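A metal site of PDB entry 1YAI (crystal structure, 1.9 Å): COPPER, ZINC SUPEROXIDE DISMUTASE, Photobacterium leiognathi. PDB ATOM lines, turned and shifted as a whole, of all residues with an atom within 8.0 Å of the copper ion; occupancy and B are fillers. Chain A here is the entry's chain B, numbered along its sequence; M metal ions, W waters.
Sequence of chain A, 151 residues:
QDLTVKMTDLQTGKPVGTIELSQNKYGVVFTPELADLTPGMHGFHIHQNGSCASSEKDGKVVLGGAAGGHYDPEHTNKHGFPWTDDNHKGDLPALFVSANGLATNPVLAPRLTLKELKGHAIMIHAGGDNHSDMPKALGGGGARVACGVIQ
A ring nitrogen (ND1) of His 45 lies close to a ring nitrogen (NE2) of His 70 (3.0 Å).
A ring nitrogen (NE2) of His 45 sits at hydrogen-bond distance from the side-chain carboxylate (OD2) of Asp 129 (3.0 Å).
The backbone NH (N) of His 125 lies within hydrogen-bond range of the backbone carbonyl oxygen (O) of Gly 43 (2.9 Å).
The backbone carbonyl oxygen (O) of Gly 142 is in hydrogen-bond range of a ring nitrogen (ND1) of His 125 (2.7 Å).
ND1 of His 125 sits close to O of Ala 143, 3.4 Å away.
A ring nitrogen (ND1) of His 47 lies within hydrogen-bond range of the backbone carbonyl oxygen of Gly 69, at 3.2 Å.
The backbone carbonyl oxygen of Gly 68 is in hydrogen-bond range of a ring nitrogen (ND1) of His 47, at 2.7 Å.
The backbone NH of His 47 sits at hydrogen-bond distance from the backbone carbonyl oxygen of Ala 121.
A ring nitrogen (ND1) of His 45 binds the copper ion (2.0 Å).
The copper ion is bound by a ring nitrogen (NE2) of His 125 (2.1 Å).
NE2 of His 47 binds the copper ion (2.1 Å).
Slightly farther from the copper ion lies NE2 of His 70 (2.8 Å).
Four residues have an atom within 4 Å of the copper ion: His 45, His 47, His 70 and His 125.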
ATOM      1  N   GLY A  43       4.827  17.309  18.566  1.00  0.00           N
ATOM      2  CA  GLY A  43       3.857  16.802  19.536  1.00  0.00           C
ATOM      3  C   GLY A  43       3.262  18.065  20.166  1.00  0.00           C
ATOM      4  O   GLY A  43       3.982  19.034  20.470  1.00  0.00           O
ATOM      5  N   PHE A  44       1.944  18.050  20.326  1.00  0.00           N
ATOM      6  CA  PHE A  44       1.133  19.158  20.789  1.00  0.00           C
ATOM      7  C   PHE A  44       0.103  18.594  21.784  1.00  0.00           C
ATOM      8  O   PHE A  44      -0.739  17.752  21.424  1.00  0.00           O
ATOM      9  CB  PHE A  44       0.483  19.697  19.514  1.00  0.00           C
ATOM     10  CG  PHE A  44      -0.244  20.972  19.656  1.00  0.00           C
ATOM     11  CD1 PHE A  44       0.327  21.983  20.431  1.00  0.00           C
ATOM     12  CD2 PHE A  44      -1.430  21.184  18.953  1.00  0.00           C
ATOM     13  CE1 PHE A  44      -0.274  23.222  20.494  1.00  0.00           C
ATOM     14  CE2 PHE A  44      -2.047  22.431  19.064  1.00  0.00           C
ATOM     15  CZ  PHE A  44      -1.489  23.427  19.848  1.00  0.00           C
ATOM     16  N   HIS A  45       0.202  19.016  23.044  1.00  0.00           N
ATOM     17  CA  HIS A  45      -0.684  18.434  24.072  1.00  0.00           C
ATOM     18  C   HIS A  45      -1.021  19.399  25.163  1.00  0.00           C
ATOM     19  O   HIS A  45      -0.256  20.301  25.437  1.00  0.00           O
ATOM     20  CB  HIS A  45       0.018  17.296  24.830  1.00  0.00           C
ATOM     21  CG  HIS A  45       0.886  16.454  23.977  1.00  0.00           C
ATOM     22  ND1 HIS A  45       2.248  16.354  24.194  1.00  0.00           N
ATOM     23  CD2 HIS A  45       0.584  15.685  22.917  1.00  0.00           C
ATOM     24  CE1 HIS A  45       2.742  15.549  23.281  1.00  0.00           C
ATOM     25  NE2 HIS A  45       1.766  15.111  22.483  1.00  0.00           N
ATOM     26  N   ILE A  46      -2.120  19.127  25.807  1.00  0.00           N
ATOM     27  CA  ILE A  46      -2.525  19.892  26.950  1.00  0.00           C
ATOM     28  C   ILE A  46      -1.978  19.173  28.138  1.00  0.00           C
ATOM     29  O   ILE A  46      -2.162  17.932  28.247  1.00  0.00           O
ATOM     30  CB  ILE A  46      -4.033  19.904  27.089  1.00  0.00           C
ATOM     31  CG1 ILE A  46      -4.709  20.534  25.845  1.00  0.00           C
ATOM     32  CG2 ILE A  46      -4.384  20.584  28.407  1.00  0.00           C
ATOM     33  CD1 ILE A  46      -4.426  22.034  25.556  1.00  0.00           C
ATOM     34  N   HIS A  47      -1.288  19.896  29.028  1.00  0.00           N
ATOM     35  CA  HIS A  47      -0.689  19.336  30.225  1.00  0.00           C
ATOM     36  C   HIS A  47      -1.495  19.631  31.482  1.00  0.00           C
ATOM     37  O   HIS A  47      -2.299  20.536  31.532  1.00  0.00           O
ATOM     38  CB  HIS A  47       0.788  19.710  30.395  1.00  0.00           C
ATOM     39  CG  HIS A  47       1.668  18.913  29.460  1.00  0.00           C
ATOM     40  ND1 HIS A  47       2.684  18.097  29.936  1.00  0.00           N
ATOM     41  CD2 HIS A  47       1.607  18.763  28.121  1.00  0.00           C
ATOM     42  CE1 HIS A  47       3.225  17.512  28.896  1.00  0.00           C
ATOM     43  NE2 HIS A  47       2.613  17.890  27.797  1.00  0.00           N
ATOM     44  N   ALA A  67       4.649  21.778  34.352  1.00  0.00           N
ATOM     45  CA  ALA A  67       3.355  21.521  33.738  1.00  0.00           C
ATOM     46  C   ALA A  67       2.848  20.117  34.059  1.00  0.00           C
ATOM     47  O   ALA A  67       1.689  19.813  33.864  1.00  0.00           O
ATOM     48  CB  ALA A  67       3.411  21.741  32.215  1.00  0.00           C
ATOM     49  N   GLY A  68       3.729  19.240  34.487  1.00  0.00           N
ATOM     50  CA  GLY A  68       3.311  17.898  34.777  1.00  0.00           C
ATOM     51  C   GLY A  68       3.066  17.113  33.494  1.00  0.00           C
ATOM     52  O   GLY A  68       3.542  17.476  32.403  1.00  0.00           O
ATOM     53  N   GLY A  69       2.371  15.990  33.638  1.00  0.00           N
ATOM     54  CA  GLY A  69       2.081  15.091  32.547  1.00  0.00           C
ATOM     55  C   GLY A  69       0.917  15.590  31.710  1.00  0.00           C
ATOM     56  O   GLY A  69       0.458  16.712  31.832  1.00  0.00           O
ATOM     57  N   HIS A  70       0.452  14.718  30.843  1.00  0.00           N
ATOM     58  CA  HIS A  70      -0.637  15.021  29.917  1.00  0.00           C
ATOM     59  C   HIS A  70      -1.967  15.192  30.643  1.00  0.00           C
ATOM     60  O   HIS A  70      -2.232  14.491  31.572  1.00  0.00           O
ATOM     61  CB  HIS A  70      -0.764  13.906  28.853  1.00  0.00           C
ATOM     62  CG  HIS A  70       0.298  14.019  27.806  1.00  0.00           C
ATOM     63  ND1 HIS A  70       0.311  13.188  26.697  1.00  0.00           N
ATOM     64  CD2 HIS A  70       1.379  14.876  27.706  1.00  0.00           C
ATOM     65  CE1 HIS A  70       1.363  13.511  25.972  1.00  0.00           C
ATOM     66  NE2 HIS A  70       2.022  14.521  26.548  1.00  0.00           N
ATOM     67  N   TYR A  71      -2.799  16.143  30.240  1.00  0.00           N
ATOM     68  CA  TYR A  71      -4.101  16.312  30.869  1.00  0.00           C
ATOM     69  C   TYR A  71      -4.863  14.979  30.771  1.00  0.00           C
ATOM     70  O   TYR A  71      -5.158  14.503  29.676  1.00  0.00           O
ATOM     71  CB  TYR A  71      -4.870  17.351  30.085  1.00  0.00           C
ATOM     72  CG  TYR A  71      -6.267  17.595  30.584  1.00  0.00           C
ATOM     73  CD1 TYR A  71      -6.539  17.822  31.928  1.00  0.00           C
ATOM     74  CD2 TYR A  71      -7.315  17.647  29.668  1.00  0.00           C
ATOM     75  CE1 TYR A  71      -7.844  18.104  32.358  1.00  0.00           C
ATOM     76  CE2 TYR A  71      -8.620  17.892  30.090  1.00  0.00           C
ATOM     77  CZ  TYR A  71      -8.878  18.121  31.436  1.00  0.00           C
ATOM     78  OH  TYR A  71     -10.149  18.342  31.845  1.00  0.00           O
ATOM     79  N   HIS A  79      -1.337   7.260  26.343  1.00  0.00           N
ATOM     80  CA  HIS A  79      -1.218   8.282  25.303  1.00  0.00           C
ATOM     81  C   HIS A  79      -1.841   7.781  23.996  1.00  0.00           C
ATOM     82  O   HIS A  79      -1.644   6.628  23.633  1.00  0.00           O
ATOM     83  CB  HIS A  79       0.246   8.700  25.063  1.00  0.00           C
ATOM     84  CG  HIS A  79       0.320   9.836  24.101  1.00  0.00           C
ATOM     85  ND1 HIS A  79      -0.041  11.107  24.463  1.00  0.00           N
ATOM     86  CD2 HIS A  79       0.697   9.851  22.801  1.00  0.00           C
ATOM     87  CE1 HIS A  79       0.125  11.875  23.394  1.00  0.00           C
ATOM     88  NE2 HIS A  79       0.570  11.147  22.378  1.00  0.00           N
ATOM     89  N   HIS A  88      -5.248   9.907  27.253  1.00  0.00           N
ATOM     90  CA  HIS A  88      -5.225  11.317  27.708  1.00  0.00           C
ATOM     91  C   HIS A  88      -6.134  12.224  26.890  1.00  0.00           C
ATOM     92  O   HIS A  88      -6.025  12.290  25.677  1.00  0.00           O
ATOM     93  CB  HIS A  88      -3.818  11.906  27.562  1.00  0.00           C
ATOM     94  CG  HIS A  88      -2.773  11.099  28.183  1.00  0.00           C
ATOM     95  ND1 HIS A  88      -1.582  10.875  27.529  1.00  0.00           N
ATOM     96  CD2 HIS A  88      -2.721  10.535  29.407  1.00  0.00           C
ATOM     97  CE1 HIS A  88      -0.831  10.203  28.362  1.00  0.00           C
ATOM     98  NE2 HIS A  88      -1.509   9.934  29.487  1.00  0.00           N
ATOM     99  N   GLY A  90      -5.939  15.248  26.890  1.00  0.00           N
ATOM    100  CA  GLY A  90      -5.129  16.357  26.419  1.00  0.00           C
ATOM    101  C   GLY A  90      -4.328  16.080  25.130  1.00  0.00           C
ATOM    102  O   GLY A  90      -3.517  16.904  24.685  1.00  0.00           O
ATOM    103  N   ASP A  91      -4.581  14.917  24.535  1.00  0.00           N
ATOM    104  CA  ASP A  91      -3.907  14.568  23.300  1.00  0.00           C
ATOM    105  C   ASP A  91      -4.469  15.264  22.040  1.00  0.00           C
ATOM    106  O   ASP A  91      -5.489  14.869  21.497  1.00  0.00           O
ATOM    107  CB  ASP A  91      -3.857  13.027  23.147  1.00  0.00           C
ATOM    108  CG  ASP A  91      -3.085  12.324  24.268  1.00  0.00           C
ATOM    109  OD1 ASP A  91      -2.227  12.900  24.969  1.00  0.00           O
ATOM    110  OD2 ASP A  91      -3.406  11.093  24.406  1.00  0.00           O
ATOM    111  N   ALA A 121      -1.761  23.883  30.848  1.00  0.00           N
ATOM    112  CA  ALA A 121      -0.684  24.357  29.977  1.00  0.00           C
ATOM    113  C   ALA A 121      -0.738  23.751  28.572  1.00  0.00           C
ATOM    114  O   ALA A 121      -1.019  22.556  28.451  1.00  0.00           O
ATOM    115  CB  ALA A 121       0.682  24.082  30.610  1.00  0.00           C
ATOM    116  N   ILE A 122      -0.512  24.560  27.540  1.00  0.00           N
ATOM    117  CA  ILE A 122      -0.428  24.050  26.172  1.00  0.00           C
ATOM    118  C   ILE A 122       1.069  23.805  25.922  1.00  0.00           C
ATOM    119  O   ILE A 122       1.868  24.699  26.120  1.00  0.00           O
ATOM    120  CB  ILE A 122      -0.941  25.031  25.138  1.00  0.00           C
ATOM    121  CG1 ILE A 122      -2.405  25.288  25.392  1.00  0.00           C
ATOM    122  CG2 ILE A 122      -0.754  24.359  23.794  1.00  0.00           C
ATOM    123  CD1 ILE A 122      -3.046  26.083  24.257  1.00  0.00           C
ATOM    124  N   MET A 123       1.448  22.611  25.498  1.00  0.00           N
ATOM    125  CA  MET A 123       2.861  22.337  25.317  1.00  0.00           C
ATOM    126  C   MET A 123       3.168  21.929  23.887  1.00  0.00           C
ATOM    127  O   MET A 123       2.418  21.157  23.315  1.00  0.00           O
ATOM    128  CB  MET A 123       3.268  21.121  26.206  1.00  0.00           C
ATOM    129  CG  MET A 123       4.756  21.014  26.454  1.00  0.00           C
ATOM    130  SD  MET A 123       5.336  22.332  27.558  1.00  0.00           S
ATOM    131  CE  MET A 123       4.413  21.956  29.096  1.00  0.00           C
ATOM    132  N   ILE A 124       4.311  22.384  23.382  1.00  0.00           N
ATOM    133  CA  ILE A 124       4.793  22.005  22.059  1.00  0.00           C
ATOM    134  C   ILE A 124       6.134  21.278  22.296  1.00  0.00           C
ATOM    135  O   ILE A 124       6.990  21.796  22.980  1.00  0.00           O
ATOM    136  CB  ILE A 124       4.994  23.243  21.152  1.00  0.00           C
ATOM    137  CG1 ILE A 124       3.694  23.983  20.818  1.00  0.00           C
ATOM    138  CG2 ILE A 124       5.783  22.887  19.885  1.00  0.00           C
ATOM    139  CD1 ILE A 124       3.895  25.175  19.864  1.00  0.00           C
ATOM    140  N   HIS A 125       6.303  20.106  21.747  1.00  0.00           N
ATOM    141  CA  HIS A 125       7.511  19.351  21.976  1.00  0.00           C
ATOM    142  C   HIS A 125       8.497  19.402  20.829  1.00  0.00           C
ATOM    143  O   HIS A 125       8.159  19.794  19.722  1.00  0.00           O
ATOM    144  CB  HIS A 125       7.136  17.870  22.230  1.00  0.00           C
ATOM    145  CG  HIS A 125       6.412  17.648  23.517  1.00  0.00           C
ATOM    146  ND1 HIS A 125       7.037  17.160  24.654  1.00  0.00           N
ATOM    147  CD2 HIS A 125       5.082  17.808  23.808  1.00  0.00           C
ATOM    148  CE1 HIS A 125       6.098  17.038  25.609  1.00  0.00           C
ATOM    149  NE2 HIS A 125       4.941  17.450  25.123  1.00  0.00           N
ATOM    150  N   ASP A 129       4.614  13.107  17.024  1.00  0.00           N
ATOM    151  CA  ASP A 129       3.636  12.346  17.795  1.00  0.00           C
ATOM    152  C   ASP A 129       3.001  11.262  16.943  1.00  0.00           C
ATOM    153  O   ASP A 129       2.270  11.519  16.004  1.00  0.00           O
ATOM    154  CB  ASP A 129       2.508  13.282  18.339  1.00  0.00           C
ATOM    155  CG  ASP A 129       1.713  12.618  19.426  1.00  0.00           C
ATOM    156  OD1 ASP A 129       1.739  11.418  19.636  1.00  0.00           O
ATOM    157  OD2 ASP A 129       0.970  13.454  20.127  1.00  0.00           O
ATOM    158  N   LEU A 138       4.651   8.512  25.131  1.00  0.00           N
ATOM    159  CA  LEU A 138       4.036   9.803  24.885  1.00  0.00           C
ATOM    160  C   LEU A 138       4.163  10.263  23.441  1.00  0.00           C
ATOM    161  O   LEU A 138       4.307  11.470  23.156  1.00  0.00           O
ATOM    162  CB  LEU A 138       4.605  10.853  25.880  1.00  0.00           C
ATOM    163  CG  LEU A 138       4.216  10.517  27.327  1.00  0.00           C
ATOM    164  CD1 LEU A 138       4.865  11.472  28.330  1.00  0.00           C
ATOM    165  CD2 LEU A 138       2.689  10.555  27.473  1.00  0.00           C
ATOM    166  N   GLY A 141       7.280  12.705  21.627  1.00  0.00           N
ATOM    167  CA  GLY A 141       7.385  14.144  21.637  1.00  0.00           C
ATOM    168  C   GLY A 141       8.704  14.618  22.223  1.00  0.00           C
ATOM    169  O   GLY A 141       9.251  15.641  21.817  1.00  0.00           O
ATOM    170  N   GLY A 142       9.230  13.879  23.186  1.00  0.00           N
ATOM    171  CA  GLY A 142      10.486  14.237  23.798  1.00  0.00           C
ATOM    172  C   GLY A 142      10.416  15.548  24.548  1.00  0.00           C
ATOM    173  O   GLY A 142       9.401  15.919  25.170  1.00  0.00           O
ATOM    174  N   ALA A 143      11.534  16.279  24.490  1.00  0.00           N
ATOM    175  CA  ALA A 143      11.651  17.558  25.190  1.00  0.00           C
ATOM    176  C   ALA A 143      10.580  18.600  24.876  1.00  0.00           C
ATOM    177  O   ALA A 143       9.983  18.659  23.797  1.00  0.00           O
ATOM    178  CB  ALA A 143      12.999  18.142  25.014  1.00  0.00           C
ATOM    179  N   ARG A 144      10.343  19.438  25.879  1.00  0.00           N
ATOM    180  CA  ARG A 144       9.369  20.521  25.800  1.00  0.00           C
ATOM    181  C   ARG A 144      10.060  21.790  25.313  1.00  0.00           C
ATOM    182  O   ARG A 144      11.102  22.196  25.849  1.00  0.00           O
ATOM    183  CB  ARG A 144       8.668  20.711  27.151  1.00  0.00           C
ATOM    184  CG  ARG A 144       8.091  19.393  27.699  1.00  0.00           C
ATOM    185  CD  ARG A 144       7.756  19.436  29.195  1.00  0.00           C
ATOM    186  NE  ARG A 144       7.293  18.115  29.660  1.00  0.00           N
ATOM    187  CZ  ARG A 144       6.424  17.891  30.651  1.00  0.00           C
ATOM    188  NH1 ARG A 144       5.912  18.893  31.369  1.00  0.00           N
ATOM    189  NH2 ARG A 144       6.083  16.654  30.938  1.00  0.00           N
HETATM  190 CU    CU M   1       3.065  17.024  25.907  1.00  0.00          CU
HETATM  191 ZN    ZN M   2      -0.995  11.992  25.858  1.00  0.00          ZN
HETATM  192  O   HOH W   1       4.931  14.933  27.476  1.00  0.00           O
